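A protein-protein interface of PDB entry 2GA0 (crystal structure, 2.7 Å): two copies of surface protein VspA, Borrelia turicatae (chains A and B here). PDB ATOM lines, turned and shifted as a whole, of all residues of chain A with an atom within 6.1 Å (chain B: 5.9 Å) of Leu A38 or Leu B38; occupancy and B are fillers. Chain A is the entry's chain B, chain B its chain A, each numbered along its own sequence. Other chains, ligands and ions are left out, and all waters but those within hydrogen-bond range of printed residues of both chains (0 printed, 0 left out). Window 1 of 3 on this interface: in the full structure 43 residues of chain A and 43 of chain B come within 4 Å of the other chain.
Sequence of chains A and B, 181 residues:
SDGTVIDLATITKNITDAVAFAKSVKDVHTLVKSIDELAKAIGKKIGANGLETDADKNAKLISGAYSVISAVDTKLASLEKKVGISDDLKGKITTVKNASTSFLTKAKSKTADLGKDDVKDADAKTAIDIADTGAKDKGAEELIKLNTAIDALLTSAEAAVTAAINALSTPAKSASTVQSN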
ATOM      1  N   LYS A  33     -22.288  23.756  32.685  1.00  0.00           N
ATOM      2  CA  LYS A  33     -22.105  22.384  33.146  1.00  0.00           C
ATOM      3  C   LYS A  33     -20.995  21.712  32.339  1.00  0.00           C
ATOM      4  O   LYS A  33     -20.167  20.997  32.895  1.00  0.00           O
ATOM      5  CB  LYS A  33     -23.392  21.620  32.900  1.00  0.00           C
ATOM      6  CG  LYS A  33     -23.853  20.694  33.983  1.00  0.00           C
ATOM      7  CD  LYS A  33     -23.893  19.242  33.471  1.00  0.00           C
ATOM      8  CE  LYS A  33     -24.660  18.316  34.434  1.00  0.00           C
ATOM      9  NZ  LYS A  33     -24.761  16.867  33.936  1.00  0.00           N
ATOM     10  N   SER A  34     -20.958  21.966  31.033  1.00  0.00           N
ATOM     11  CA  SER A  34     -19.999  21.306  30.147  1.00  0.00           C
ATOM     12  C   SER A  34     -18.534  21.531  30.553  1.00  0.00           C
ATOM     13  O   SER A  34     -17.649  20.761  30.123  1.00  0.00           O
ATOM     14  CB  SER A  34     -20.229  21.719  28.677  1.00  0.00           C
ATOM     15  OG  SER A  34     -19.531  22.915  28.356  1.00  0.00           O
ATOM     16  N   ILE A  35     -18.263  22.551  31.379  1.00  0.00           N
ATOM     17  CA  ILE A  35     -16.884  22.788  31.760  1.00  0.00           C
ATOM     18  C   ILE A  35     -16.503  21.638  32.654  1.00  0.00           C
ATOM     19  O   ILE A  35     -15.324  21.342  32.821  1.00  0.00           O
ATOM     20  CB  ILE A  35     -16.671  24.159  32.451  1.00  0.00           C
ATOM     21  CG1 ILE A  35     -17.165  25.316  31.567  1.00  0.00           C
ATOM     22  CG2 ILE A  35     -15.207  24.360  32.808  1.00  0.00           C
ATOM     23  CD1 ILE A  35     -16.536  25.382  30.194  1.00  0.00           C
ATOM     24  N   ASP A  36     -17.492  20.963  33.226  1.00  0.00           N
ATOM     25  CA  ASP A  36     -17.172  19.844  34.100  1.00  0.00           C
ATOM     26  C   ASP A  36     -16.653  18.718  33.274  1.00  0.00           C
ATOM     27  O   ASP A  36     -15.822  17.915  33.763  1.00  0.00           O
ATOM     28  CB  ASP A  36     -18.357  19.336  34.893  1.00  0.00           C
ATOM     29  CG  ASP A  36     -19.045  20.401  35.624  1.00  0.00           C
ATOM     30  OD1 ASP A  36     -18.428  21.462  35.858  1.00  0.00           O
ATOM     31  OD2 ASP A  36     -20.235  20.266  35.996  1.00  0.00           O
ATOM     32  N   GLU A  37     -17.137  18.638  32.035  1.00  0.00           N
ATOM     33  CA  GLU A  37     -16.667  17.567  31.150  1.00  0.00           C
ATOM     34  C   GLU A  37     -15.239  17.883  30.737  1.00  0.00           C
ATOM     35  O   GLU A  37     -14.400  16.960  30.693  1.00  0.00           O
ATOM     36  CB  GLU A  37     -17.521  17.353  29.877  1.00  0.00           C
ATOM     37  CG  GLU A  37     -19.014  17.117  30.056  1.00  0.00           C
ATOM     38  CD  GLU A  37     -19.363  16.103  31.132  1.00  0.00           C
ATOM     39  OE1 GLU A  37     -20.478  16.270  31.679  1.00  0.00           O
ATOM     40  OE2 GLU A  37     -18.564  15.152  31.427  1.00  0.00           O
ATOM     41  N   LEU A  38     -14.948  19.164  30.458  1.00  0.00           N
ATOM     42  CA  LEU A  38     -13.591  19.556  30.079  1.00  0.00           C
ATOM     43  C   LEU A  38     -12.595  19.317  31.229  1.00  0.00           C
ATOM     44  O   LEU A  38     -11.455  18.864  31.009  1.00  0.00           O
ATOM     45  CB  LEU A  38     -13.503  21.008  29.565  1.00  0.00           C
ATOM     46  CG  LEU A  38     -14.376  21.326  28.351  1.00  0.00           C
ATOM     47  CD1 LEU A  38     -14.359  22.793  28.106  1.00  0.00           C
ATOM     48  CD2 LEU A  38     -13.949  20.536  27.102  1.00  0.00           C
ATOM     49  N   ALA A  39     -13.010  19.616  32.452  1.00  0.00           N
ATOM     50  CA  ALA A  39     -12.150  19.372  33.596  1.00  0.00           C
ATOM     51  C   ALA A  39     -11.756  17.898  33.707  1.00  0.00           C
ATOM     52  O   ALA A  39     -10.619  17.578  34.122  1.00  0.00           O
ATOM     53  CB  ALA A  39     -12.782  19.863  34.900  1.00  0.00           C
ATOM     54  N   LYS A  40     -12.667  16.996  33.334  1.00  0.00           N
ATOM     55  CA  LYS A  40     -12.337  15.564  33.371  1.00  0.00           C
ATOM     56  C   LYS A  40     -11.171  15.260  32.415  1.00  0.00           C
ATOM     57  O   LYS A  40     -10.538  14.207  32.527  1.00  0.00           O
ATOM     58  CB  LYS A  40     -13.516  14.674  32.968  1.00  0.00           C
ATOM     59  CG  LYS A  40     -14.826  14.948  33.638  1.00  0.00           C
ATOM     60  CD  LYS A  40     -15.800  13.844  33.364  1.00  0.00           C
ATOM     61  CE  LYS A  40     -16.955  14.009  34.237  1.00  0.00           C
ATOM     62  NZ  LYS A  40     -18.184  13.429  33.665  1.00  0.00           N
ATOM     63  N   ALA A  41     -10.911  16.158  31.466  1.00  0.00           N
ATOM     64  CA  ALA A  41      -9.890  15.921  30.469  1.00  0.00           C
ATOM     65  C   ALA A  41      -8.518  16.481  30.831  1.00  0.00           C
ATOM     66  O   ALA A  41      -7.539  16.154  30.179  1.00  0.00           O
ATOM     67  CB  ALA A  41     -10.343  16.432  29.137  1.00  0.00           C
ATOM     68  N   ILE A  42      -8.449  17.302  31.876  1.00  0.00           N
ATOM     69  CA  ILE A  42      -7.178  17.821  32.379  1.00  0.00           C
ATOM     70  C   ILE A  42      -6.174  16.692  32.520  1.00  0.00           C
ATOM     71  O   ILE A  42      -6.449  15.696  33.168  1.00  0.00           O
ATOM     72  CB  ILE A  42      -7.373  18.450  33.756  1.00  0.00           C
ATOM     73  CG1 ILE A  42      -8.220  19.722  33.672  1.00  0.00           C
ATOM     74  CG2 ILE A  42      -6.025  18.719  34.418  1.00  0.00           C
ATOM     75  CD1 ILE A  42      -8.482  20.336  35.020  1.00  0.00           C
ATOM     76  N   LYS A  60      -4.408  24.701  26.003  1.00  0.00           N
ATOM     77  CA  LYS A  60      -5.421  24.739  24.949  1.00  0.00           C
ATOM     78  C   LYS A  60      -6.752  24.179  25.446  1.00  0.00           C
ATOM     79  O   LYS A  60      -7.821  24.580  24.951  1.00  0.00           O
ATOM     80  CB  LYS A  60      -4.916  24.003  23.713  1.00  0.00           C
ATOM     81  CG  LYS A  60      -4.231  24.914  22.703  1.00  0.00           C
ATOM     82  CD  LYS A  60      -2.756  24.946  22.877  1.00  0.00           C
ATOM     83  CE  LYS A  60      -2.233  26.345  22.764  1.00  0.00           C
ATOM     84  NZ  LYS A  60      -0.880  26.257  22.150  1.00  0.00           N
ATOM     85  N   LEU A  61      -6.698  23.265  26.428  1.00  0.00           N
ATOM     86  CA  LEU A  61      -7.923  22.840  27.081  1.00  0.00           C
ATOM     87  C   LEU A  61      -8.549  24.013  27.846  1.00  0.00           C
ATOM     88  O   LEU A  61      -9.755  24.262  27.693  1.00  0.00           O
ATOM     89  CB  LEU A  61      -7.723  21.620  27.984  1.00  0.00           C
ATOM     90  CG  LEU A  61      -8.887  21.146  28.887  1.00  0.00           C
ATOM     91  CD1 LEU A  61     -10.083  20.704  28.087  1.00  0.00           C
ATOM     92  CD2 LEU A  61      -8.389  20.024  29.726  1.00  0.00           C
ATOM     93  N   SER A  63      -8.137  27.008  27.120  1.00  0.00           N
ATOM     94  CA  SER A  63      -8.578  27.928  26.081  1.00  0.00           C
ATOM     95  C   SER A  63      -9.974  27.502  25.629  1.00  0.00           C
ATOM     96  O   SER A  63     -10.842  28.356  25.417  1.00  0.00           O
ATOM     97  CB  SER A  63      -7.588  27.966  24.926  1.00  0.00           C
ATOM     98  OG  SER A  63      -6.403  28.600  25.334  1.00  0.00           O
ATOM     99  N   GLY A  64     -10.181  26.184  25.521  1.00  0.00           N
ATOM    100  CA  GLY A  64     -11.476  25.634  25.192  1.00  0.00           C
ATOM    101  C   GLY A  64     -12.543  26.132  26.147  1.00  0.00           C
ATOM    102  O   GLY A  64     -13.539  26.711  25.711  1.00  0.00           O
ATOM    103  N   ALA A  65     -12.317  25.933  27.450  1.00  0.00           N
ATOM    104  CA  ALA A  65     -13.223  26.361  28.498  1.00  0.00           C
ATOM    105  C   ALA A  65     -13.490  27.843  28.274  1.00  0.00           C
ATOM    106  O   ALA A  65     -14.653  28.294  28.185  1.00  0.00           O
ATOM    107  CB  ALA A  65     -12.597  26.106  29.848  1.00  0.00           C
ATOM    108  N   SER A  67     -13.280  29.621  25.679  1.00  0.00           N
ATOM    109  CA  SER A  67     -14.093  29.834  24.489  1.00  0.00           C
ATOM    110  C   SER A  67     -15.580  29.568  24.779  1.00  0.00           C
ATOM    111  O   SER A  67     -16.451  30.306  24.309  1.00  0.00           O
ATOM    112  CB  SER A  67     -13.575  28.940  23.372  1.00  0.00           C
ATOM    113  OG  SER A  67     -14.346  29.069  22.197  1.00  0.00           O
ATOM    114  N   VAL A  68     -15.849  28.539  25.592  1.00  0.00           N
ATOM    115  CA  VAL A  68     -17.216  28.143  25.897  1.00  0.00           C
ATOM    116  C   VAL A  68     -17.860  29.203  26.765  1.00  0.00           C
ATOM    117  O   VAL A  68     -18.978  29.609  26.499  1.00  0.00           O
ATOM    118  CB  VAL A  68     -17.315  26.736  26.549  1.00  0.00           C
ATOM    119  CG1 VAL A  68     -18.633  26.564  27.259  1.00  0.00           C
ATOM    120  CG2 VAL A  68     -17.178  25.679  25.496  1.00  0.00           C
ATOM    121  N   ILE A 128     -10.640  25.782  35.954  1.00  0.00           N
ATOM    122  CA  ILE A 128     -11.847  25.243  35.374  1.00  0.00           C
ATOM    123  C   ILE A 128     -12.441  24.041  36.088  1.00  0.00           C
ATOM    124  O   ILE A 128     -13.393  23.435  35.576  1.00  0.00           O
ATOM    125  CB  ILE A 128     -11.604  24.896  33.921  1.00  0.00           C
ATOM    126  CG1 ILE A 128     -10.644  23.711  33.775  1.00  0.00           C
ATOM    127  CG2 ILE A 128     -11.050  26.072  33.221  1.00  0.00           C
ATOM    128  CD1 ILE A 128     -10.931  22.885  32.461  1.00  0.00           C
ATOM    129  N   SER B  34     -21.242  22.831  21.287  1.00  0.00           N
ATOM    130  CA  SER B  34     -20.161  23.384  22.074  1.00  0.00           C
ATOM    131  C   SER B  34     -18.804  22.978  21.522  1.00  0.00           C
ATOM    132  O   SER B  34     -17.804  23.695  21.720  1.00  0.00           O
ATOM    133  CB  SER B  34     -20.299  23.030  23.545  1.00  0.00           C
ATOM    134  OG  SER B  34     -19.787  21.765  23.850  1.00  0.00           O
ATOM    135  N   ILE B  35     -18.758  21.875  20.787  1.00  0.00           N
ATOM    136  CA  ILE B  35     -17.516  21.517  20.144  1.00  0.00           C
ATOM    137  C   ILE B  35     -17.008  22.631  19.185  1.00  0.00           C
ATOM    138  O   ILE B  35     -15.787  22.786  19.002  1.00  0.00           O
ATOM    139  CB  ILE B  35     -17.619  20.124  19.500  1.00  0.00           C
ATOM    140  CG1 ILE B  35     -18.273  19.166  20.486  1.00  0.00           C
ATOM    141  CG2 ILE B  35     -16.240  19.576  19.058  1.00  0.00           C
ATOM    142  CD1 ILE B  35     -17.601  19.014  21.853  1.00  0.00           C
ATOM    143  N   ASP B  36     -17.931  23.415  18.631  1.00  0.00           N
ATOM    144  CA  ASP B  36     -17.583  24.554  17.794  1.00  0.00           C
ATOM    145  C   ASP B  36     -16.910  25.659  18.599  1.00  0.00           C
ATOM    146  O   ASP B  36     -16.056  26.393  18.073  1.00  0.00           O
ATOM    147  CB  ASP B  36     -18.822  25.110  17.098  1.00  0.00           C
ATOM    148  CG  ASP B  36     -19.494  24.080  16.194  1.00  0.00           C
ATOM    149  OD1 ASP B  36     -18.991  22.928  16.108  1.00  0.00           O
ATOM    150  OD2 ASP B  36     -20.521  24.319  15.522  1.00  0.00           O
ATOM    151  N   GLU B  37     -17.256  25.769  19.873  1.00  0.00           N
ATOM    152  CA  GLU B  37     -16.569  26.748  20.686  1.00  0.00           C
ATOM    153  C   GLU B  37     -15.159  26.247  20.944  1.00  0.00           C
ATOM    154  O   GLU B  37     -14.221  27.037  20.847  1.00  0.00           O
ATOM    155  CB  GLU B  37     -17.315  27.090  21.976  1.00  0.00           C
ATOM    156  CG  GLU B  37     -18.768  27.495  21.739  1.00  0.00           C
ATOM    157  CD  GLU B  37     -18.905  28.609  20.717  1.00  0.00           C
ATOM    158  OE1 GLU B  37     -19.893  28.623  19.947  1.00  0.00           O
ATOM    159  OE2 GLU B  37     -18.023  29.491  20.672  1.00  0.00           O
ATOM    160  N   LEU B  38     -15.008  24.942  21.210  1.00  0.00           N
ATOM    161  CA  LEU B  38     -13.693  24.381  21.527  1.00  0.00           C
ATOM    162  C   LEU B  38     -12.748  24.494  20.340  1.00  0.00           C
ATOM    163  O   LEU B  38     -11.547  24.808  20.512  1.00  0.00           O
ATOM    164  CB  LEU B  38     -13.771  22.927  21.984  1.00  0.00           C
ATOM    165  CG  LEU B  38     -14.683  22.628  23.161  1.00  0.00           C
ATOM    166  CD1 LEU B  38     -14.613  21.171  23.497  1.00  0.00           C
ATOM    167  CD2 LEU B  38     -14.246  23.482  24.319  1.00  0.00           C
ATOM    168  N   ALA B  39     -13.284  24.273  19.145  1.00  0.00           N
ATOM    169  CA  ALA B  39     -12.502  24.407  17.936  1.00  0.00           C
ATOM    170  C   ALA B  39     -11.978  25.843  17.747  1.00  0.00           C
ATOM    171  O   ALA B  39     -10.881  26.032  17.242  1.00  0.00           O
ATOM    172  CB  ALA B  39     -13.287  23.936  16.744  1.00  0.00           C
ATOM    173  N   LYS B  40     -12.730  26.846  18.187  1.00  0.00           N
ATOM    174  CA  LYS B  40     -12.227  28.224  18.104  1.00  0.00           C
ATOM    175  C   LYS B  40     -10.950  28.372  18.948  1.00  0.00           C
ATOM    176  O   LYS B  40     -10.155  29.312  18.704  1.00  0.00           O
ATOM    177  CB  LYS B  40     -13.271  29.269  18.542  1.00  0.00           C
ATOM    178  CG  LYS B  40     -14.486  29.484  17.612  1.00  0.00           C
ATOM    179  CD  LYS B  40     -15.582  30.152  18.391  1.00  0.00           C
ATOM    180  CE  LYS B  40     -16.899  30.120  17.698  1.00  0.00           C
ATOM    181  NZ  LYS B  40     -17.829  31.125  18.349  1.00  0.00           N
ATOM    182  N   ALA B  41     -10.729  27.446  19.894  1.00  0.00           N
ATOM    183  CA  ALA B  41      -9.571  27.554  20.760  1.00  0.00           C
ATOM    184  C   ALA B  41      -8.297  26.860  20.257  1.00  0.00           C
ATOM    185  O   ALA B  41      -7.240  27.007  20.859  1.00  0.00           O
ATOM    186  CB  ALA B  41      -9.906  27.083  22.164  1.00  0.00           C
ATOM    187  N   ILE B  42      -8.405  26.085  19.181  1.00  0.00           N
ATOM    188  CA  ILE B  42      -7.275  25.346  18.619  1.00  0.00           C
ATOM    189  C   ILE B  42      -6.168  26.306  18.330  1.00  0.00           C
ATOM    190  O   ILE B  42      -6.383  27.311  17.678  1.00  0.00           O
ATOM    191  CB  ILE B  42      -7.667  24.663  17.320  1.00  0.00           C
ATOM    192  CG1 ILE B  42      -8.692  23.564  17.600  1.00  0.00           C
ATOM    193  CG2 ILE B  42      -6.449  24.086  16.633  1.00  0.00           C
ATOM    194  CD1 ILE B  42      -9.241  22.928  16.392  1.00  0.00           C
ATOM    195  N   LEU B  61      -6.974  19.815  24.490  1.00  0.00           N
ATOM    196  CA  LEU B  61      -8.188  20.368  23.968  1.00  0.00           C
ATOM    197  C   LEU B  61      -8.995  19.281  23.252  1.00  0.00           C
ATOM    198  O   LEU B  61     -10.209  19.208  23.451  1.00  0.00           O
ATOM    199  CB  LEU B  61      -7.897  21.550  23.066  1.00  0.00           C
ATOM    200  CG  LEU B  61      -9.128  22.183  22.432  1.00  0.00           C
ATOM    201  CD1 LEU B  61     -10.059  22.756  23.466  1.00  0.00           C
ATOM    202  CD2 LEU B  61      -8.767  23.231  21.332  1.00  0.00           C
ATOM    203  N   GLY B  64     -10.675  17.222  25.622  1.00  0.00           N
ATOM    204  CA  GLY B  64     -11.856  17.925  26.090  1.00  0.00           C
ATOM    205  C   GLY B  64     -13.061  17.609  25.220  1.00  0.00           C
ATOM    206  O   GLY B  64     -14.125  17.187  25.684  1.00  0.00           O
ATOM    207  N   ALA B  65     -12.882  17.794  23.929  1.00  0.00           N
ATOM    208  CA  ALA B  65     -13.960  17.552  22.996  1.00  0.00           C
ATOM    209  C   ALA B  65     -14.374  16.095  23.136  1.00  0.00           C
ATOM    210  O   ALA B  65     -15.564  15.768  23.233  1.00  0.00           O
ATOM    211  CB  ALA B  65     -13.545  17.946  21.537  1.00  0.00           C
ATOM    212  N   SER B  67     -14.166  14.181  25.749  1.00  0.00           N
ATOM    213  CA  SER B  67     -14.902  14.093  26.989  1.00  0.00           C
ATOM    214  C   SER B  67     -16.327  14.555  26.814  1.00  0.00           C
ATOM    215  O   SER B  67     -17.258  13.904  27.303  1.00  0.00           O
ATOM    216  CB  SER B  67     -14.259  14.983  28.030  1.00  0.00           C
ATOM    217  OG  SER B  67     -14.709  14.643  29.329  1.00  0.00           O
ATOM    218  N   VAL B  68     -16.504  15.682  26.122  1.00  0.00           N
ATOM    219  CA  VAL B  68     -17.843  16.221  25.910  1.00  0.00           C
ATOM    220  C   VAL B  68     -18.721  15.252  25.096  1.00  0.00           C
ATOM    221  O   VAL B  68     -19.846  14.991  25.456  1.00  0.00           O
ATOM    222  CB  VAL B  68     -17.843  17.702  25.325  1.00  0.00           C
ATOM    223  CG1 VAL B  68     -19.271  18.172  24.948  1.00  0.00           C
ATOM    224  CG2 VAL B  68     -17.192  18.692  26.322  1.00  0.00           C
ATOM    225  N   ILE B 128     -12.088  17.972  15.290  1.00  0.00           N
ATOM    226  CA  ILE B 128     -13.137  18.674  16.024  1.00  0.00           C
ATOM    227  C   ILE B 128     -13.626  19.942  15.380  1.00  0.00           C
ATOM    228  O   ILE B 128     -14.406  20.649  16.003  1.00  0.00           O
ATOM    229  CB  ILE B 128     -12.689  19.028  17.473  1.00  0.00           C
ATOM    230  CG1 ILE B 128     -11.586  20.067  17.471  1.00  0.00           C
ATOM    231  CG2 ILE B 128     -12.280  17.797  18.231  1.00  0.00           C
ATOM    232  CD1 ILE B 128     -11.592  20.911  18.714  1.00  0.00           C
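Leu A38 touches its own counterpart, Leu B38. Lys A40 touches Ser B67, and with the chains exchanged Ser A67 touches Lys B40. Leu A61 touches its own counterpart, Leu B61. Leu A61 touches Gly B64, and with the chains exchanged Gly A64 touches Leu B61. Of the 18 pairs that touch across the chains among the printed residues, 16 have their exchanged pair printed and touching as well.
Leu A38 touches Leu B38. Gly B64 touches Leu A38. CB of Ala A41 touches N of Gly B64, 3.6 Å away. Leu B61 touches Lys A60 (CD1 to O, 3.2 Å). Leu B61 touches Leu A61. CD1 of Leu A61 touches CA of Gly B64, at 3.9 Å. O of Gly A64 touches CD2 of Leu B38 (3.6 Å). CA of Gly A64 touches CD1 of Leu B61 (3.6 Å). Ser A67 touches Lys B40. CB of Glu B37 touches CG2 of Val A68, 3.8 Å away.
Printed residues of chain A that touch a printed residue of chain B: Glu A37, Leu A38, Lys A40, Ala A41, Lys A60, Leu A61, Ser A63, Gly A64, Ser A67 and Val A68. Along chain A the printed residues that touch a printed residue of chain B span positions 37 to 68. Printed residues of chain B that touch a printed residue of chain A: Glu B37, Leu B38, Lys B40, Ala B41, Leu B61, Gly B64, Ser B67 and Val B68. Hydrophobic or aromatic side chains of chain B that line the printed part of chain A: Leu B38, Ala B41, Leu B61 and Val B68. Along chain B the printed residues that touch a printed residue of chain A span positions 37 to 68. Among the printed residues, no Asp or Glu carboxylate lies within 4 Å of a Lys or Arg side-chain nitrogen of the other chain.
O of Glu B37 is in hydrogen-bond range of OG of Ser A67 (2.4 Å). The side-chain hydroxyl (OG) of Ser B67 is in hydrogen-bond range of the backbone carbonyl oxygen (O) of Glu A37 (2.7 Å).
Of the printed residues of chain B, Leu A38 touches Leu B38 (3.7 Å), Gly B64 (3.5 Å) and Val B68 (3.8 Å). Printed residues of chain B within 4 Å of Ser A67: Glu B37 (2.4 Å) and Lys B40 (3.8 Å). Of the printed residues of chain A, Ser B67 touches Glu A37 (2.7 Å) and Lys A40 (3.8 Å). The nearest residue of chain B that does not touch Leu A38 is Ala B65 (4.3 Å). The nearest residue of chain A that does not touch Leu B38 is Ser A67 (4.3 Å).
The side-chain amino group (NZ) of Lys A40 lies within salt-bridge range of the side-chain carboxylate (OE2) of Glu A37 (2.8 Å). The side-chain amino group (NZ) of Lys B40 is in salt-bridge range of the side-chain carboxylate (OE2) of Glu B37.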
